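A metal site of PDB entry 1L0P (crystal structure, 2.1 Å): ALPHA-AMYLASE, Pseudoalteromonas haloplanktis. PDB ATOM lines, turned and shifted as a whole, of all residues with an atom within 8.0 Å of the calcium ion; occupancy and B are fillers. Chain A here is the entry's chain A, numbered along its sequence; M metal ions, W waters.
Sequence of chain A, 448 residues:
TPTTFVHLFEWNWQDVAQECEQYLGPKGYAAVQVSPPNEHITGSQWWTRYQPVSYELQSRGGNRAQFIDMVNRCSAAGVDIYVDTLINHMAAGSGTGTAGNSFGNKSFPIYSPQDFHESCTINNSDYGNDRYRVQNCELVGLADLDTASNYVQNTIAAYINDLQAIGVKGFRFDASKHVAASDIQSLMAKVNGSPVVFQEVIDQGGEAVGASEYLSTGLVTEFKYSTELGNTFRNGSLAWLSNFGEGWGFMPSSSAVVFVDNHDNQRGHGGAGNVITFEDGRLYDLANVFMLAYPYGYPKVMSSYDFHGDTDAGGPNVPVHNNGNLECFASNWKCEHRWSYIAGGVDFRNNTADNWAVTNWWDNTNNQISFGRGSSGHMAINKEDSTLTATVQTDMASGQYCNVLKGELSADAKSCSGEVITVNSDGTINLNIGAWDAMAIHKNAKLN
O of Asn 88 is in hydrogen-bond range of N of Leu 145. A ring nitrogen (ND1) of His 89 lies within hydrogen-bond range of the side-chain amide nitrogen (ND2) of Asn 88 (3.0 Å). A ring nitrogen (ND1) of His 178 is in hydrogen-bond range of the backbone carbonyl oxygen (O) of Val 134 (3.0 Å). The backbone carbonyl oxygen (O) of Asp 144 lies within hydrogen-bond range of the backbone NH (N) of His 117 (2.8 Å). O of Lys 177 sits at hydrogen-bond distance from NE2 of Gln 135 (3.2 Å).
Of the 26 residues printed, 4 come within 4 Å of the calcium ion.
Water W3 binds the calcium ion (2.3 Å). The calcium ion is bound by OD1 of Asn 88, 2.3 Å away. The calcium ion is bound by O of His 178, 2.4 Å away. OD2 of Asp 144 binds the calcium ion, at 2.4 Å. Water W1 is bound to the calcium ion, 2.5 Å away. The side-chain carboxylate (OD1) of Asp 144 is bound to the calcium ion (2.6 Å). Water W2 binds the calcium ion. The calcium ion is bound by O of Gln 135 (2.6 Å). The calcium ion has eight donor atoms within binding distance.
Water W3 lies within hydrogen-bond range of O of Asn 88 (2.7 Å) and O of Leu 145 (2.7 Å).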
ATOM      1  N   ILE A  87      21.328  18.860  18.555  1.00  0.00           N
ATOM      2  CA  ILE A  87      21.631  17.446  18.787  1.00  0.00           C
ATOM      3  C   ILE A  87      23.031  16.999  18.412  1.00  0.00           C
ATOM      4  O   ILE A  87      23.467  15.912  18.799  1.00  0.00           O
ATOM      5  CB  ILE A  87      20.636  16.535  18.033  1.00  0.00           C
ATOM      6  CG1 ILE A  87      20.713  16.811  16.533  1.00  0.00           C
ATOM      7  CG2 ILE A  87      19.230  16.743  18.582  1.00  0.00           C
ATOM      8  CD1 ILE A  87      20.030  15.798  15.685  1.00  0.00           C
ATOM      9  N   ASN A  88      23.765  17.858  17.699  1.00  0.00           N
ATOM     10  CA  ASN A  88      25.110  17.522  17.224  1.00  0.00           C
ATOM     11  C   ASN A  88      26.296  17.941  18.087  1.00  0.00           C
ATOM     12  O   ASN A  88      27.294  17.208  18.162  1.00  0.00           O
ATOM     13  CB  ASN A  88      25.298  18.124  15.825  1.00  0.00           C
ATOM     14  CG  ASN A  88      26.663  17.809  15.214  1.00  0.00           C
ATOM     15  OD1 ASN A  88      26.943  16.671  14.835  1.00  0.00           O
ATOM     16  ND2 ASN A  88      27.505  18.829  15.091  1.00  0.00           N
ATOM     17  N   HIS A  89      26.174  19.051  18.793  1.00  0.00           N
ATOM     18  CA  HIS A  89      27.335  19.573  19.501  1.00  0.00           C
ATOM     19  C   HIS A  89      27.093  20.441  20.724  1.00  0.00           C
ATOM     20  O   HIS A  89      25.965  20.790  21.055  1.00  0.00           O
ATOM     21  CB  HIS A  89      28.113  20.424  18.491  1.00  0.00           C
ATOM     22  CG  HIS A  89      27.273  21.477  17.855  1.00  0.00           C
ATOM     23  ND1 HIS A  89      26.614  21.284  16.649  1.00  0.00           N
ATOM     24  CD2 HIS A  89      26.876  22.694  18.297  1.00  0.00           C
ATOM     25  CE1 HIS A  89      25.853  22.328  16.390  1.00  0.00           C
ATOM     26  NE2 HIS A  89      25.991  23.195  17.374  1.00  0.00           N
ATOM     27  N   HIS A 117      33.283  12.973  20.362  1.00  0.00           N
ATOM     28  CA  HIS A 117      34.141  12.300  19.407  1.00  0.00           C
ATOM     29  C   HIS A 117      35.498  12.971  19.542  1.00  0.00           C
ATOM     30  O   HIS A 117      35.591  14.125  19.977  1.00  0.00           O
ATOM     31  CB  HIS A 117      33.637  12.531  17.988  1.00  0.00           C
ATOM     32  CG  HIS A 117      32.370  11.797  17.665  1.00  0.00           C
ATOM     33  ND1 HIS A 117      31.358  12.348  16.914  1.00  0.00           N
ATOM     34  CD2 HIS A 117      31.984  10.533  17.955  1.00  0.00           C
ATOM     35  CE1 HIS A 117      30.400  11.472  16.752  1.00  0.00           C
ATOM     36  NE2 HIS A 117      30.749  10.358  17.370  1.00  0.00           N
ATOM     37  N   ILE A 122      36.135  19.488  10.254  1.00  0.00           N
ATOM     38  CA  ILE A 122      35.421  19.190   9.021  1.00  0.00           C
ATOM     39  C   ILE A 122      35.926  20.192   7.987  1.00  0.00           C
ATOM     40  O   ILE A 122      35.921  21.398   8.229  1.00  0.00           O
ATOM     41  CB  ILE A 122      33.878  19.383   9.141  1.00  0.00           C
ATOM     42  CG1 ILE A 122      33.251  18.355  10.074  1.00  0.00           C
ATOM     43  CG2 ILE A 122      33.244  19.239   7.766  1.00  0.00           C
ATOM     44  CD1 ILE A 122      31.755  18.542  10.271  1.00  0.00           C
ATOM     45  N   TYR A 132      32.227  10.112   7.025  1.00  0.00           N
ATOM     46  CA  TYR A 132      32.747   9.851   8.363  1.00  0.00           C
ATOM     47  C   TYR A 132      33.165  11.157   9.010  1.00  0.00           C
ATOM     48  O   TYR A 132      32.783  11.448  10.135  1.00  0.00           O
ATOM     49  CB  TYR A 132      33.932   8.876   8.334  1.00  0.00           C
ATOM     50  CG  TYR A 132      34.525   8.628   9.707  1.00  0.00           C
ATOM     51  CD1 TYR A 132      33.996   7.655  10.558  1.00  0.00           C
ATOM     52  CD2 TYR A 132      35.593   9.401  10.167  1.00  0.00           C
ATOM     53  CE1 TYR A 132      34.506   7.469  11.850  1.00  0.00           C
ATOM     54  CE2 TYR A 132      36.115   9.223  11.458  1.00  0.00           C
ATOM     55  CZ  TYR A 132      35.558   8.251  12.294  1.00  0.00           C
ATOM     56  OH  TYR A 132      36.099   8.050  13.551  1.00  0.00           O
ATOM     57  N   ARG A 133      33.940  11.961   8.278  1.00  0.00           N
ATOM     58  CA  ARG A 133      34.404  13.258   8.780  1.00  0.00           C
ATOM     59  C   ARG A 133      33.257  14.249   8.992  1.00  0.00           C
ATOM     60  O   ARG A 133      33.239  14.964   9.981  1.00  0.00           O
ATOM     61  CB  ARG A 133      35.436  13.862   7.851  1.00  0.00           C
ATOM     62  CG  ARG A 133      36.784  13.161   7.940  1.00  0.00           C
ATOM     63  CD  ARG A 133      37.892  14.046   7.399  1.00  0.00           C
ATOM     64  NE  ARG A 133      38.966  14.155   8.378  1.00  0.00           N
ATOM     65  CZ  ARG A 133      39.448  15.304   8.820  1.00  0.00           C
ATOM     66  NH1 ARG A 133      38.962  16.442   8.362  1.00  0.00           N
ATOM     67  NH2 ARG A 133      40.416  15.313   9.720  1.00  0.00           N
ATOM     68  N   VAL A 134      32.305  14.274   8.059  1.00  0.00           N
ATOM     69  CA  VAL A 134      31.142  15.164   8.173  1.00  0.00           C
ATOM     70  C   VAL A 134      30.359  14.907   9.473  1.00  0.00           C
ATOM     71  O   VAL A 134      29.927  15.839  10.161  1.00  0.00           O
ATOM     72  CB  VAL A 134      30.166  14.942   6.960  1.00  0.00           C
ATOM     73  CG1 VAL A 134      28.812  15.627   7.211  1.00  0.00           C
ATOM     74  CG2 VAL A 134      30.788  15.477   5.683  1.00  0.00           C
ATOM     75  N   GLN A 135      30.205  13.635   9.830  1.00  0.00           N
ATOM     76  CA  GLN A 135      29.436  13.247  10.999  1.00  0.00           C
ATOM     77  C   GLN A 135      30.218  13.015  12.299  1.00  0.00           C
ATOM     78  O   GLN A 135      29.621  12.970  13.381  1.00  0.00           O
ATOM     79  CB  GLN A 135      28.553  12.051  10.653  1.00  0.00           C
ATOM     80  CG  GLN A 135      27.633  12.339   9.470  1.00  0.00           C
ATOM     81  CD  GLN A 135      26.686  11.205   9.122  1.00  0.00           C
ATOM     82  OE1 GLN A 135      26.962  10.042   9.390  1.00  0.00           O
ATOM     83  NE2 GLN A 135      25.545  11.544   8.495  1.00  0.00           N
ATOM     84  N   ASN A 136      31.540  12.890  12.215  1.00  0.00           N
ATOM     85  CA  ASN A 136      32.333  12.664  13.430  1.00  0.00           C
ATOM     86  C   ASN A 136      33.273  13.796  13.772  1.00  0.00           C
ATOM     87  O   ASN A 136      33.687  13.912  14.922  1.00  0.00           O
ATOM     88  CB  ASN A 136      33.067  11.330  13.359  1.00  0.00           C
ATOM     89  CG  ASN A 136      32.117  10.150  13.372  1.00  0.00           C
ATOM     90  OD1 ASN A 136      31.700   9.687  14.434  1.00  0.00           O
ATOM     91  ND2 ASN A 136      31.721   9.688  12.192  1.00  0.00           N
ATOM     92  N   CYS A 137      33.595  14.646  12.796  1.00  0.00           N
ATOM     93  CA  CYS A 137      34.484  15.769  13.090  1.00  0.00           C
ATOM     94  C   CYS A 137      33.714  17.017  13.512  1.00  0.00           C
ATOM     95  O   CYS A 137      32.479  17.042  13.460  1.00  0.00           O
ATOM     96  CB  CYS A 137      35.404  16.055  11.902  1.00  0.00           C
ATOM     97  SG  CYS A 137      36.553  14.686  11.573  1.00  0.00           S
ATOM     98  N   GLU A 138      34.444  18.031  13.937  1.00  0.00           N
ATOM     99  CA  GLU A 138      33.861  19.273  14.418  1.00  0.00           C
ATOM    100  C   GLU A 138      33.454  20.272  13.367  1.00  0.00           C
ATOM    101  O   GLU A 138      34.195  20.559  12.422  1.00  0.00           O
ATOM    102  CB  GLU A 138      34.797  19.934  15.418  1.00  0.00           C
ATOM    103  CG  GLU A 138      35.069  19.080  16.638  1.00  0.00           C
ATOM    104  CD  GLU A 138      36.210  19.585  17.499  1.00  0.00           C
ATOM    105  OE1 GLU A 138      36.997  20.450  17.038  1.00  0.00           O
ATOM    106  OE2 GLU A 138      36.343  19.102  18.646  1.00  0.00           O
ATOM    107  N   LEU A 139      32.246  20.797  13.525  1.00  0.00           N
ATOM    108  CA  LEU A 139      31.694  21.810  12.650  1.00  0.00           C
ATOM    109  C   LEU A 139      32.175  23.116  13.264  1.00  0.00           C
ATOM    110  O   LEU A 139      31.773  23.463  14.379  1.00  0.00           O
ATOM    111  CB  LEU A 139      30.163  21.734  12.672  1.00  0.00           C
ATOM    112  CG  LEU A 139      29.334  22.793  11.950  1.00  0.00           C
ATOM    113  CD1 LEU A 139      29.653  22.799  10.452  1.00  0.00           C
ATOM    114  CD2 LEU A 139      27.852  22.492  12.186  1.00  0.00           C
ATOM    115  N   LEU A 142      33.051  23.351  17.095  1.00  0.00           N
ATOM    116  CA  LEU A 142      32.065  22.929  18.090  1.00  0.00           C
ATOM    117  C   LEU A 142      32.314  21.476  18.509  1.00  0.00           C
ATOM    118  O   LEU A 142      32.434  20.598  17.661  1.00  0.00           O
ATOM    119  CB  LEU A 142      30.655  23.062  17.502  1.00  0.00           C
ATOM    120  CG  LEU A 142      29.971  24.438  17.371  1.00  0.00           C
ATOM    121  CD1 LEU A 142      30.926  25.577  17.604  1.00  0.00           C
ATOM    122  CD2 LEU A 142      29.303  24.544  16.027  1.00  0.00           C
ATOM    123  N   ALA A 143      32.376  21.236  19.826  1.00  0.00           N
ATOM    124  CA  ALA A 143      32.616  19.888  20.360  1.00  0.00           C
ATOM    125  C   ALA A 143      31.560  18.934  19.826  1.00  0.00           C
ATOM    126  O   ALA A 143      30.374  19.093  20.092  1.00  0.00           O
ATOM    127  CB  ALA A 143      32.613  19.920  21.898  1.00  0.00           C
ATOM    128  N   ASP A 144      31.990  17.914  19.085  1.00  0.00           N
ATOM    129  CA  ASP A 144      31.061  16.980  18.472  1.00  0.00           C
ATOM    130  C   ASP A 144      30.654  15.870  19.426  1.00  0.00           C
ATOM    131  O   ASP A 144      31.454  15.011  19.761  1.00  0.00           O
ATOM    132  CB  ASP A 144      31.671  16.414  17.200  1.00  0.00           C
ATOM    133  CG  ASP A 144      30.625  15.971  16.207  1.00  0.00           C
ATOM    134  OD1 ASP A 144      29.876  16.836  15.699  1.00  0.00           O
ATOM    135  OD2 ASP A 144      30.558  14.775  15.905  1.00  0.00           O
ATOM    136  N   LEU A 145      29.389  15.889  19.830  1.00  0.00           N
ATOM    137  CA  LEU A 145      28.855  14.896  20.746  1.00  0.00           C
ATOM    138  C   LEU A 145      28.905  13.481  20.168  1.00  0.00           C
ATOM    139  O   LEU A 145      28.722  13.290  18.953  1.00  0.00           O
ATOM    140  CB  LEU A 145      27.393  15.203  21.078  1.00  0.00           C
ATOM    141  CG  LEU A 145      27.005  16.255  22.113  1.00  0.00           C
ATOM    142  CD1 LEU A 145      25.494  16.509  22.050  1.00  0.00           C
ATOM    143  CD2 LEU A 145      27.421  15.777  23.476  1.00  0.00           C
ATOM    144  N   ASP A 146      29.150  12.502  21.020  1.00  0.00           N
ATOM    145  CA  ASP A 146      29.146  11.108  20.578  1.00  0.00           C
ATOM    146  C   ASP A 146      27.665  10.671  20.618  1.00  0.00           C
ATOM    147  O   ASP A 146      27.189  10.116  21.620  1.00  0.00           O
ATOM    148  CB  ASP A 146      30.001  10.236  21.495  1.00  0.00           C
ATOM    149  CG  ASP A 146      30.037   8.778  21.055  1.00  0.00           C
ATOM    150  OD1 ASP A 146      29.423   8.400  20.022  1.00  0.00           O
ATOM    151  OD2 ASP A 146      30.694   7.995  21.764  1.00  0.00           O
ATOM    152  N   THR A 147      26.956  10.950  19.531  1.00  0.00           N
ATOM    153  CA  THR A 147      25.538  10.642  19.442  1.00  0.00           C
ATOM    154  C   THR A 147      25.170   9.148  19.407  1.00  0.00           C
ATOM    155  O   THR A 147      23.988   8.792  19.427  1.00  0.00           O
ATOM    156  CB  THR A 147      24.902  11.406  18.266  1.00  0.00           C
ATOM    157  OG1 THR A 147      25.675  11.188  17.085  1.00  0.00           O
ATOM    158  CG2 THR A 147      24.905  12.895  18.574  1.00  0.00           C
ATOM    159  N   ALA A 175      21.568  20.973  12.657  1.00  0.00           N
ATOM    160  CA  ALA A 175      22.736  20.281  12.093  1.00  0.00           C
ATOM    161  C   ALA A 175      22.563  18.773  12.004  1.00  0.00           C
ATOM    162  O   ALA A 175      23.484  18.007  12.367  1.00  0.00           O
ATOM    163  CB  ALA A 175      23.993  20.634  12.917  1.00  0.00           C
ATOM    164  N   SER A 176      21.402  18.337  11.526  1.00  0.00           N
ATOM    165  CA  SER A 176      21.106  16.915  11.420  1.00  0.00           C
ATOM    166  C   SER A 176      22.028  16.170  10.487  1.00  0.00           C
ATOM    167  O   SER A 176      22.311  14.985  10.703  1.00  0.00           O
ATOM    168  CB  SER A 176      19.655  16.687  10.990  1.00  0.00           C
ATOM    169  OG  SER A 176      18.791  17.001  12.056  1.00  0.00           O
ATOM    170  N   LYS A 177      22.524  16.849   9.453  1.00  0.00           N
ATOM    171  CA  LYS A 177      23.441  16.217   8.507  1.00  0.00           C
ATOM    172  C   LYS A 177      24.709  15.726   9.200  1.00  0.00           C
ATOM    173  O   LYS A 177      25.271  14.700   8.814  1.00  0.00           O
ATOM    174  CB  LYS A 177      23.803  17.185   7.369  1.00  0.00           C
ATOM    175  CG  LYS A 177      24.712  16.546   6.316  1.00  0.00           C
ATOM    176  CD  LYS A 177      24.677  17.312   5.011  1.00  0.00           C
ATOM    177  CE  LYS A 177      25.483  18.579   5.094  1.00  0.00           C
ATOM    178  NZ  LYS A 177      25.303  19.362   3.843  1.00  0.00           N
ATOM    179  N   HIS A 178      25.103  16.424  10.254  1.00  0.00           N
ATOM    180  CA  HIS A 178      26.314  16.076  10.994  1.00  0.00           C
ATOM    181  C   HIS A 178      26.104  14.973  12.022  1.00  0.00           C
ATOM    182  O   HIS A 178      26.996  14.692  12.812  1.00  0.00           O
ATOM    183  CB  HIS A 178      26.932  17.337  11.610  1.00  0.00           C
ATOM    184  CG  HIS A 178      27.250  18.387  10.590  1.00  0.00           C
ATOM    185  ND1 HIS A 178      28.490  18.507  10.003  1.00  0.00           N
ATOM    186  CD2 HIS A 178      26.464  19.320   9.989  1.00  0.00           C
ATOM    187  CE1 HIS A 178      28.465  19.474   9.098  1.00  0.00           C
ATOM    188  NE2 HIS A 178      27.247  19.977   9.071  1.00  0.00           N
ATOM    189  N   VAL A 179      24.934  14.342  11.980  1.00  0.00           N
ATOM    190  CA  VAL A 179      24.631  13.229  12.880  1.00  0.00           C
ATOM    191  C   VAL A 179      24.110  12.089  12.025  1.00  0.00           C
ATOM    192  O   VAL A 179      23.211  12.294  11.201  1.00  0.00           O
ATOM    193  CB  VAL A 179      23.568  13.598  13.957  1.00  0.00           C
ATOM    194  CG1 VAL A 179      23.204  12.355  14.794  1.00  0.00           C
ATOM    195  CG2 VAL A 179      24.082  14.704  14.850  1.00  0.00           C
ATOM    196  N   ALA A 180      24.656  10.893  12.214  1.00  0.00           N
ATOM    197  CA  ALA A 180      24.223   9.710  11.460  1.00  0.00           C
ATOM    198  C   ALA A 180      22.724   9.478  11.628  1.00  0.00           C
ATOM    199  O   ALA A 180      22.198   9.528  12.753  1.00  0.00           O
ATOM    200  CB  ALA A 180      25.009   8.477  11.904  1.00  0.00           C
ATOM    201  N   ASP A 183      21.762   7.230  14.347  1.00  0.00           N
ATOM    202  CA  ASP A 183      21.875   7.769  15.714  1.00  0.00           C
ATOM    203  C   ASP A 183      20.569   8.490  16.059  1.00  0.00           C
ATOM    204  O   ASP A 183      20.102   8.408  17.200  1.00  0.00           O
ATOM    205  CB  ASP A 183      23.037   8.758  15.854  1.00  0.00           C
ATOM    206  CG  ASP A 183      24.402   8.069  15.880  1.00  0.00           C
ATOM    207  OD1 ASP A 183      24.466   6.826  15.915  1.00  0.00           O
ATOM    208  OD2 ASP A 183      25.414   8.800  15.881  1.00  0.00           O
HETATM  209 CA    CA M   1      28.436  14.890  14.743  1.00  0.00          CA
HETATM  210  O   HOH W   1      27.530  12.655  15.236  1.00  0.00           O
HETATM  211  O   HOH W   2      29.903  16.120  12.966  1.00  0.00           O
HETATM  212  O   HOH W   3      27.681  14.802  16.909  1.00  0.00           O
